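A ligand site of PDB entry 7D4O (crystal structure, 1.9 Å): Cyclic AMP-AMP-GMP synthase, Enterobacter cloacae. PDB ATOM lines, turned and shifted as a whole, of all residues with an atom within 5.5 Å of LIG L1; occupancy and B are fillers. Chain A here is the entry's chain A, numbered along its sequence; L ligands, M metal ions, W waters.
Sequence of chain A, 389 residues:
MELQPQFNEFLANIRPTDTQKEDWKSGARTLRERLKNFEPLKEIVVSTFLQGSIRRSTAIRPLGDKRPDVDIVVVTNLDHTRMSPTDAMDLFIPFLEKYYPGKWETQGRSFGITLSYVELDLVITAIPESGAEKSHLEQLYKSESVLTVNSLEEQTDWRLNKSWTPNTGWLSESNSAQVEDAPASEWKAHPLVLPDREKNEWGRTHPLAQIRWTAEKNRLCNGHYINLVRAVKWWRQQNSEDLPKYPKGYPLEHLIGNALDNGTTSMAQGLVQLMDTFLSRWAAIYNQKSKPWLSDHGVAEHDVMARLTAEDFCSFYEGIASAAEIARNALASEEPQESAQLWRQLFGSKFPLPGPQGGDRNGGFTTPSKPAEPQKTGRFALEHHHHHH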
ATOM      1  N   GLN A  51      20.338  20.871   9.285  1.00  0.00           N
ATOM      2  CA  GLN A  51      21.433  20.099   9.897  1.00  0.00           C
ATOM      3  C   GLN A  51      22.582  19.978   8.895  1.00  0.00           C
ATOM      4  O   GLN A  51      22.667  20.743   7.920  1.00  0.00           O
ATOM      5  CB  GLN A  51      20.919  18.721  10.359  1.00  0.00           C
ATOM      6  CG  GLN A  51      20.459  17.817   9.163  1.00  0.00           C
ATOM      7  CD  GLN A  51      20.689  16.322   9.475  1.00  0.00           C
ATOM      8  OE1 GLN A  51      21.206  15.973  10.536  1.00  0.00           O
ATOM      9  NE2 GLN A  51      20.270  15.447   8.563  1.00  0.00           N
ATOM     10  N   ASP A  71      21.087  19.482   4.196  1.00  0.00           N
ATOM     11  CA  ASP A  71      20.455  18.431   4.998  1.00  0.00           C
ATOM     12  C   ASP A  71      19.391  19.003   5.926  1.00  0.00           C
ATOM     13  O   ASP A  71      19.626  19.990   6.620  1.00  0.00           O
ATOM     14  CB  ASP A  71      21.533  17.711   5.803  1.00  0.00           C
ATOM     15  CG  ASP A  71      22.562  17.062   4.877  1.00  0.00           C
ATOM     16  OD1 ASP A  71      22.191  16.047   4.214  1.00  0.00           O
ATOM     17  OD2 ASP A  71      23.683  17.597   4.749  1.00  0.00           O
ATOM     18  N   VAL A  73      16.312  17.668   8.874  1.00  0.00           N
ATOM     19  CA  VAL A  73      15.719  16.618   9.699  1.00  0.00           C
ATOM     20  C   VAL A  73      14.245  16.946   9.906  1.00  0.00           C
ATOM     21  O   VAL A  73      13.912  18.060  10.302  1.00  0.00           O
ATOM     22  CB  VAL A  73      16.407  16.500  11.074  1.00  0.00           C
ATOM     23  CG1 VAL A  73      15.645  15.482  11.966  1.00  0.00           C
ATOM     24  CG2 VAL A  73      17.864  16.108  10.898  1.00  0.00           C
ATOM     25  N   ARG A 109      17.481   6.314   2.055  1.00  0.00           N
ATOM     26  CA  ARG A 109      17.112   6.656   3.428  1.00  0.00           C
ATOM     27  C   ARG A 109      16.640   8.090   3.557  1.00  0.00           C
ATOM     28  O   ARG A 109      16.372   8.519   4.695  1.00  0.00           O
ATOM     29  CB  ARG A 109      18.308   6.459   4.376  1.00  0.00           C
ATOM     30  CG  ARG A 109      19.441   7.478   4.096  1.00  0.00           C
ATOM     31  CD  ARG A 109      19.786   8.268   5.397  1.00  0.00           C
ATOM     32  NE  ARG A 109      20.226   7.381   6.492  1.00  0.00           N
ATOM     33  CZ  ARG A 109      21.464   6.905   6.627  1.00  0.00           C
ATOM     34  NH1 ARG A 109      22.409   7.178   5.698  1.00  0.00           N
ATOM     35  NH2 ARG A 109      21.765   6.118   7.667  1.00  0.00           N
ATOM     36  N   ASP A 121      17.972  17.551   1.313  1.00  0.00           N
ATOM     37  CA  ASP A 121      18.195  16.131   1.612  1.00  0.00           C
ATOM     38  C   ASP A 121      17.496  15.919   2.958  1.00  0.00           C
ATOM     39  O   ASP A 121      18.058  16.251   4.006  1.00  0.00           O
ATOM     40  CB  ASP A 121      19.698  15.844   1.688  1.00  0.00           C
ATOM     41  CG  ASP A 121      20.026  14.403   1.781  1.00  0.00           C
ATOM     42  OD1 ASP A 121      19.085  13.603   1.886  1.00  0.00           O
ATOM     43  OD2 ASP A 121      21.234  14.065   1.789  1.00  0.00           O
ATOM     44  N   VAL A 123      15.723  13.810   5.936  1.00  0.00           N
ATOM     45  CA  VAL A 123      15.620  12.525   6.609  1.00  0.00           C
ATOM     46  C   VAL A 123      14.473  12.583   7.617  1.00  0.00           C
ATOM     47  O   VAL A 123      14.284  13.599   8.297  1.00  0.00           O
ATOM     48  CB  VAL A 123      16.949  12.112   7.272  1.00  0.00           C
ATOM     49  CG1 VAL A 123      17.990  11.778   6.224  1.00  0.00           C
ATOM     50  CG2 VAL A 123      17.456  13.187   8.202  1.00  0.00           C
ATOM     51  N   LEU A 194      16.816   7.238  12.797  1.00  0.00           N
ATOM     52  CA  LEU A 194      16.572   7.517  11.387  1.00  0.00           C
ATOM     53  C   LEU A 194      16.703   6.207  10.610  1.00  0.00           C
ATOM     54  O   LEU A 194      17.150   5.192  11.184  1.00  0.00           O
ATOM     55  CB  LEU A 194      17.572   8.574  10.862  1.00  0.00           C
ATOM     56  CG  LEU A 194      18.889   8.028  10.252  1.00  0.00           C
ATOM     57  CD1 LEU A 194      19.728   9.193   9.639  1.00  0.00           C
ATOM     58  CD2 LEU A 194      19.727   7.260  11.295  1.00  0.00           C
ATOM     59  N   PRO A 195      16.342   6.164   9.326  1.00  0.00           N
ATOM     60  CA  PRO A 195      16.504   4.920   8.558  1.00  0.00           C
ATOM     61  C   PRO A 195      17.983   4.607   8.377  1.00  0.00           C
ATOM     62  O   PRO A 195      18.782   5.500   8.083  1.00  0.00           O
ATOM     63  CB  PRO A 195      15.855   5.245   7.199  1.00  0.00           C
ATOM     64  CG  PRO A 195      14.943   6.417   7.468  1.00  0.00           C
ATOM     65  CD  PRO A 195      15.625   7.198   8.553  1.00  0.00           C
ATOM     66  N   ASP A 196      18.339   3.331   8.506  1.00  0.00           N
ATOM     67  CA  ASP A 196      19.688   2.929   8.106  1.00  0.00           C
ATOM     68  C   ASP A 196      19.843   3.150   6.598  1.00  0.00           C
ATOM     69  O   ASP A 196      18.862   3.232   5.861  1.00  0.00           O
ATOM     70  CB  ASP A 196      19.910   1.445   8.425  1.00  0.00           C
ATOM     71  CG  ASP A 196      20.211   1.198   9.904  1.00  0.00           C
ATOM     72  OD1 ASP A 196      20.581   2.153  10.625  1.00  0.00           O
ATOM     73  OD2 ASP A 196      20.089   0.027  10.339  1.00  0.00           O
ATOM     74  N   ARG A 197      21.096   3.273   6.137  1.00  0.00           N
ATOM     75  CA  ARG A 197      21.295   3.714   4.742  1.00  0.00           C
ATOM     76  C   ARG A 197      20.674   2.748   3.741  1.00  0.00           C
ATOM     77  O   ARG A 197      20.048   3.183   2.747  1.00  0.00           O
ATOM     78  CB  ARG A 197      22.801   3.838   4.435  1.00  0.00           C
ATOM     79  CG  ARG A 197      23.070   4.466   3.030  1.00  0.00           C
ATOM     80  CD  ARG A 197      24.575   4.307   2.641  1.00  0.00           C
ATOM     81  NE  ARG A 197      25.436   5.175   3.428  1.00  0.00           N
ATOM     82  CZ  ARG A 197      26.666   5.522   3.050  1.00  0.00           C
ATOM     83  NH1 ARG A 197      27.403   6.318   3.813  1.00  0.00           N
ATOM     84  NH2 ARG A 197      27.145   5.058   1.891  1.00  0.00           N
ATOM     85  N   GLU A 198      20.880   1.440   3.934  1.00  0.00           N
ATOM     86  CA  GLU A 198      20.552   0.448   2.910  1.00  0.00           C
ATOM     87  C   GLU A 198      19.525  -0.589   3.336  1.00  0.00           C
ATOM     88  O   GLU A 198      19.206  -1.498   2.546  1.00  0.00           O
ATOM     89  CB  GLU A 198      21.834  -0.297   2.478  1.00  0.00           C
ATOM     90  CG  GLU A 198      22.829   0.605   1.784  1.00  0.00           C
ATOM     91  CD  GLU A 198      22.436   0.892   0.326  1.00  0.00           C
ATOM     92  OE1 GLU A 198      21.230   0.808  -0.032  1.00  0.00           O
ATOM     93  OE2 GLU A 198      23.361   1.176  -0.468  1.00  0.00           O
ATOM     94  N   GLY A 203      18.303   3.277  12.899  1.00  0.00           N
ATOM     95  CA  GLY A 203      19.611   3.467  13.521  1.00  0.00           C
ATOM     96  C   GLY A 203      19.635   4.776  14.298  1.00  0.00           C
ATOM     97  O   GLY A 203      18.798   5.643  14.067  1.00  0.00           O
ATOM     98  N   ARG A 204      20.584   4.958  15.195  1.00  0.00           N
ATOM     99  CA  ARG A 204      20.632   6.165  16.014  1.00  0.00           C
ATOM    100  C   ARG A 204      21.433   7.249  15.308  1.00  0.00           C
ATOM    101  O   ARG A 204      22.434   6.970  14.638  1.00  0.00           O
ATOM    102  CB  ARG A 204      21.278   5.862  17.368  1.00  0.00           C
ATOM    103  CG  ARG A 204      20.418   4.801  18.167  1.00  0.00           C
ATOM    104  CD  ARG A 204      21.263   4.096  19.256  1.00  0.00           C
ATOM    105  NE  ARG A 204      21.060   4.839  20.481  1.00  0.00           N
ATOM    106  CZ  ARG A 204      21.620   4.569  21.644  1.00  0.00           C
ATOM    107  NH1 ARG A 204      22.461   3.537  21.758  1.00  0.00           N
ATOM    108  NH2 ARG A 204      21.354   5.339  22.697  1.00  0.00           N
ATOM    109  N   THR A 205      21.008   8.498  15.517  1.00  0.00           N
ATOM    110  CA  THR A 205      21.747   9.675  15.043  1.00  0.00           C
ATOM    111  C   THR A 205      21.501  10.813  16.019  1.00  0.00           C
ATOM    112  O   THR A 205      20.392  10.967  16.544  1.00  0.00           O
ATOM    113  CB  THR A 205      21.307  10.074  13.619  1.00  0.00           C
ATOM    114  OG1 THR A 205      22.071  11.185  13.149  1.00  0.00           O
ATOM    115  CG2 THR A 205      19.808  10.467  13.580  1.00  0.00           C
ATOM    116  N   HIS A 206      22.503  11.646  16.285  1.00  0.00           N
ATOM    117  CA  HIS A 206      22.317  12.728  17.245  1.00  0.00           C
ATOM    118  C   HIS A 206      22.838  14.025  16.649  1.00  0.00           C
ATOM    119  O   HIS A 206      23.873  14.534  17.054  1.00  0.00           O
ATOM    120  CB  HIS A 206      23.016  12.401  18.572  1.00  0.00           C
ATOM    121  CG  HIS A 206      22.433  13.151  19.761  1.00  0.00           C
ATOM    122  ND1 HIS A 206      21.699  14.306  19.622  1.00  0.00           N
ATOM    123  CD2 HIS A 206      22.483  12.881  21.090  1.00  0.00           C
ATOM    124  CE1 HIS A 206      21.329  14.728  20.824  1.00  0.00           C
ATOM    125  NE2 HIS A 206      21.788  13.882  21.724  1.00  0.00           N
ATOM    126  N   PRO A 207      22.153  14.554  15.631  1.00  0.00           N
ATOM    127  CA  PRO A 207      22.659  15.753  14.960  1.00  0.00           C
ATOM    128  C   PRO A 207      22.788  16.972  15.888  1.00  0.00           C
ATOM    129  O   PRO A 207      23.711  17.773  15.735  1.00  0.00           O
ATOM    130  CB  PRO A 207      21.659  15.966  13.819  1.00  0.00           C
ATOM    131  CG  PRO A 207      20.410  15.192  14.258  1.00  0.00           C
ATOM    132  CD  PRO A 207      20.957  13.996  14.977  1.00  0.00           C
ATOM    133  N   ASP A 296      31.683   8.519  17.300  1.00  0.00           N
ATOM    134  CA  ASP A 296      30.889   9.667  16.883  1.00  0.00           C
ATOM    135  C   ASP A 296      30.573  10.588  18.055  1.00  0.00           C
ATOM    136  O   ASP A 296      30.233  10.122  19.157  1.00  0.00           O
ATOM    137  CB  ASP A 296      29.605   9.161  16.237  1.00  0.00           C
ATOM    138  CG  ASP A 296      28.734  10.272  15.739  1.00  0.00           C
ATOM    139  OD1 ASP A 296      29.207  11.123  14.976  1.00  0.00           O
ATOM    140  OD2 ASP A 296      27.543  10.269  16.106  1.00  0.00           O
ATOM    141  N   VAL A 299      26.613   9.802  18.733  1.00  0.00           N
ATOM    142  CA  VAL A 299      26.252   8.438  19.175  1.00  0.00           C
ATOM    143  C   VAL A 299      27.575   7.736  19.490  1.00  0.00           C
ATOM    144  O   VAL A 299      28.274   7.282  18.580  1.00  0.00           O
ATOM    145  CB  VAL A 299      25.456   7.682  18.096  1.00  0.00           C
ATOM    146  CG1 VAL A 299      25.101   6.238  18.513  1.00  0.00           C
ATOM    147  CG2 VAL A 299      24.157   8.438  17.743  1.00  0.00           C
ATOM    148  N   HIS A 302      28.925   4.454  17.901  1.00  0.00           N
ATOM    149  CA  HIS A 302      29.127   4.381  16.459  1.00  0.00           C
ATOM    150  C   HIS A 302      30.551   4.758  16.050  1.00  0.00           C
ATOM    151  O   HIS A 302      31.088   5.751  16.530  1.00  0.00           O
ATOM    152  CB  HIS A 302      28.157   5.310  15.722  1.00  0.00           C
ATOM    153  CG  HIS A 302      26.758   4.794  15.656  1.00  0.00           C
ATOM    154  ND1 HIS A 302      25.735   5.511  15.069  1.00  0.00           N
ATOM    155  CD2 HIS A 302      26.218   3.615  16.052  1.00  0.00           C
ATOM    156  CE1 HIS A 302      24.624   4.795  15.109  1.00  0.00           C
ATOM    157  NE2 HIS A 302      24.882   3.648  15.709  1.00  0.00           N
ATOM    158  N   ARG A 307      32.508   2.792   7.385  1.00  0.00           N
ATOM    159  CA  ARG A 307      32.473   2.421   5.957  1.00  0.00           C
ATOM    160  C   ARG A 307      33.788   2.722   5.235  1.00  0.00           C
ATOM    161  O   ARG A 307      33.908   2.393   4.047  1.00  0.00           O
ATOM    162  CB  ARG A 307      31.314   3.136   5.250  1.00  0.00           C
ATOM    163  CG  ARG A 307      29.911   2.619   5.623  1.00  0.00           C
ATOM    164  CD  ARG A 307      28.807   3.384   4.869  1.00  0.00           C
ATOM    165  NE  ARG A 307      27.486   2.792   5.134  1.00  0.00           N
ATOM    166  CZ  ARG A 307      26.966   1.822   4.383  1.00  0.00           C
ATOM    167  NH1 ARG A 307      27.646   1.356   3.314  1.00  0.00           N
ATOM    168  NH2 ARG A 307      25.779   1.287   4.686  1.00  0.00           N
HETATM  169  P1  LIG L   1      24.526   3.073   7.991  1.00  0.00           P
HETATM  170  O1  LIG L   1      25.131   2.753   9.355  1.00  0.00           O
HETATM  171  O2  LIG L   1      23.261   3.879   8.041  1.00  0.00           O
HETATM  172  O3  LIG L   1      24.530   1.872   7.031  1.00  0.00           O
HETATM  173  P2  LIG L   1      25.816   5.595   7.095  1.00  0.00           P
HETATM  174  O4  LIG L   1      27.302   5.843   6.918  1.00  0.00           O
HETATM  175  O5  LIG L   1      24.970   6.149   5.992  1.00  0.00           O
HETATM  176  O6  LIG L   1      25.670   4.004   7.307  1.00  0.00           O
HETATM  177  O7  LIG L   1      25.386   6.266   8.507  1.00  0.00           O
HETATM  178  C1  LIG L   1      26.143   6.154   9.730  1.00  0.00           C
HETATM  179  C2  LIG L   1      25.477   7.084  10.763  1.00  0.00           C
HETATM  180  O8  LIG L   1      25.564   8.452  10.339  1.00  0.00           O
HETATM  181  C3  LIG L   1      23.976   6.865  10.897  1.00  0.00           C
HETATM  182  O9  LIG L   1      23.728   5.804  11.815  1.00  0.00           O
HETATM  183  C4  LIG L   1      23.494   8.189  11.440  1.00  0.00           C
HETATM  184  O10 LIG L   1      23.906   8.344  12.817  1.00  0.00           O
HETATM  185  C5  LIG L   1      24.411   9.162  10.753  1.00  0.00           C
HETATM  186  N1  LIG L   1      23.789   9.708   9.518  1.00  0.00           N
HETATM  187  C6  LIG L   1      24.047   9.281   8.253  1.00  0.00           C
HETATM  188  N2  LIG L   1      23.336  10.046   7.372  1.00  0.00           N
HETATM  189  C7  LIG L   1      22.642  10.972   8.083  1.00  0.00           C
HETATM  190  C8  LIG L   1      21.691  12.045   7.758  1.00  0.00           C
HETATM  191  N3  LIG L   1      21.376  12.294   6.459  1.00  0.00           N
HETATM  192  N4  LIG L   1      21.175  12.776   8.755  1.00  0.00           N
HETATM  193  C9  LIG L   1      21.500  12.519  10.034  1.00  0.00           C
HETATM  194  N5  LIG L   1      22.338  11.526  10.401  1.00  0.00           N
HETATM  195  C10 LIG L   1      22.939  10.739   9.482  1.00  0.00           C
HETATM  196  P1  LG2 L   2      28.560  17.530   2.740  1.00  0.00           P
HETATM  197  O1  LG2 L   2      29.555  16.749   1.899  1.00  0.00           O
HETATM  198  O2  LG2 L   2      27.120  17.199   2.456  1.00  0.00           O
HETATM  199  O3  LG2 L   2      28.882  19.013   2.789  1.00  0.00           O
HETATM  200  P2  LG2 L   2      27.781  16.655   5.362  1.00  0.00           P
HETATM  201  O4  LG2 L   2      28.453  16.722   6.685  1.00  0.00           O
HETATM  202  O5  LG2 L   2      26.534  17.453   5.144  1.00  0.00           O
HETATM  203  O6  LG2 L   2      28.882  16.951   4.230  1.00  0.00           O
HETATM  204  P3  LG2 L   2      26.244  14.297   4.494  1.00  0.00           P
HETATM  205  O7  LG2 L   2      26.837  13.119   3.784  1.00  0.00           O
HETATM  206  O8  LG2 L   2      25.369  15.283   3.773  1.00  0.00           O
HETATM  207  O9  LG2 L   2      27.495  15.075   5.133  1.00  0.00           O
HETATM  208  O10 LG2 L   2      25.492  13.780   5.809  1.00  0.00           O
HETATM  209  C1  LG2 L   2      24.533  14.592   6.502  1.00  0.00           C
HETATM  210  C2  LG2 L   2      24.837  14.474   7.999  1.00  0.00           C
HETATM  211  O11 LG2 L   2      24.668  13.124   8.443  1.00  0.00           O
HETATM  212  C3  LG2 L   2      26.295  14.768   8.371  1.00  0.00           C
HETATM  213  O12 LG2 L   2      26.630  16.156   8.425  1.00  0.00           O
HETATM  214  C4  LG2 L   2      26.394  14.079   9.721  1.00  0.00           C
HETATM  215  O13 LG2 L   2      25.715  14.876  10.704  1.00  0.00           O
HETATM  216  C5  LG2 L   2      25.567  12.825   9.505  1.00  0.00           C
HETATM  217  N1  LG2 L   2      26.479  11.766   9.046  1.00  0.00           N
HETATM  218  C6  LG2 L   2      26.717  11.375   7.767  1.00  0.00           C
HETATM  219  N2  LG2 L   2      27.641  10.373   7.751  1.00  0.00           N
HETATM  220  C7  LG2 L   2      28.021  10.165   9.056  1.00  0.00           C
HETATM  221  C8  LG2 L   2      28.962   9.296   9.765  1.00  0.00           C
HETATM  222  N3  LG2 L   2      29.740   8.370   9.109  1.00  0.00           N
HETATM  223  N4  LG2 L   2      29.030   9.387  11.125  1.00  0.00           N
HETATM  224  C9  LG2 L   2      28.278  10.262  11.823  1.00  0.00           C
HETATM  225  N5  LG2 L   2      27.403  11.094  11.220  1.00  0.00           N
HETATM  226  C10 LG2 L   2      27.251  11.084   9.873  1.00  0.00           C
HETATM  227 MG    MG M   1      23.258  14.874   2.538  1.00  0.00          MG
HETATM  228  O   HOH W   1      25.675  -0.415   7.858  1.00  0.00           O
HETATM  229  O   HOH W   2      29.052   4.516   8.427  1.00  0.00           O
HETATM  230  O   HOH W   3      29.459   7.442   6.377  1.00  0.00           O
HETATM  231  O   HOH W   4      27.730   2.173   9.134  1.00  0.00           O
HETATM  232  O   HOH W   5      26.460   8.033  14.145  1.00  0.00           O
HETATM  233  O   HOH W   6      22.460   0.250   5.985  1.00  0.00           O
HETATM  234  O   HOH W   7      25.149   3.408  11.967  1.00  0.00           O
HETATM  235  O   HOH W   8      20.026  14.787   5.487  1.00  0.00           O
HETATM  236  O   HOH W   9      21.959   4.330  10.252  1.00  0.00           O
HETATM  237  O   HOH W  10      20.860  11.394   3.508  1.00  0.00           O
HETATM  238  O   HOH W  11      24.350  10.344   4.770  1.00  0.00           O
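NE of Arg 197 is in salt-bridge range of O5 of LIG L1, at 2.8 Å. N of Arg 197 is in hydrogen-bond range of O2 of LIG L1, 2.9 Å away. The backbone carbonyl oxygen (O) of Arg 204 lies within hydrogen-bond range of an oxygen (O10) of LIG L1. A nitrogen (N4) of LIG L1 sits at hydrogen-bond distance from the side-chain amide nitrogen (NE2) of Gln 51, at 2.8 Å. The guanidinium group of Arg 109 lies within salt-bridge range of an oxygen (O2) of LIG L1 (2.7 Å). OG1 of Thr 205 sits at hydrogen-bond distance from N5 of LIG L1, 2.8 Å away. The guanidinium group (NH2) of Arg 307 is in salt-bridge range of an oxygen (O3) of LIG L1 (2.7 Å).
The backbone carbonyl oxygen (O) of Leu 194 sits at hydrogen-bond distance from the backbone NH (N) of Gly 203 (2.8 Å). The backbone carbonyl oxygen of His 302 lies within hydrogen-bond range of the backbone NH of Asp 296 (2.9 Å). O of Asp 71 is in hydrogen-bond range of N of Gln 51. The guanidinium group of Arg 109 lies within hydrogen-bond range of the backbone carbonyl oxygen of Pro 195, 2.9 Å away. OD1 of Asp 196 sits close to N of Gly 203 (3.4 Å).
Residues that only touch LIG L1: Val 123 (3.4 Å), Leu 194 (3.6 Å), Asp 196 (3.7 Å) and His 302 (3.6 Å). Ten residues have an atom within 4 Å of LIG L1: Gln 51, Arg 109, Val 123, Leu 194, Asp 196, Arg 197, Arg 204, Thr 205, His 302 and Arg 307. The nearest printed residue that does not touch LIG L1 is Asp 71 (4.4 Å).
Water W9 lies within hydrogen-bond range of the side-chain carboxylate (OD1) of Asp 196 (2.6 Å), an oxygen (O2) of LIG L1 (2.6 Å) and the guanidinium group (NH2) of Arg 109 (3.1 Å). Water W3 lies within hydrogen-bond range of O4 of LIG L1 (2.7 Å), N3 of LG2 L2 (2.9 Å) and NH1 of Arg 197 (3.5 Å). Water W6 lies within hydrogen-bond range of an oxygen (O3) of LIG L1 (2.8 Å), the backbone NH (N) of Glu 198 (2.8 Å) and the backbone NH (N) of Arg 197 (3.3 Å). Water W5 lies within hydrogen-bond range of ND1 of His 302 (2.8 Å), O10 of LIG L1 (2.9 Å) and OD2 of Asp 296 (3.2 Å). Water W8 lies within hydrogen-bond range of the backbone carbonyl oxygen of Asp 121 (2.9 Å), a nitrogen (N3) of LIG L1 (3.0 Å) and the side-chain amide nitrogen of Gln 51 (3.2 Å). Water W10 lies within hydrogen-bond range of N3 of LIG L1 (3.1 Å) and OD1 of Asp 121 (3.3 Å).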
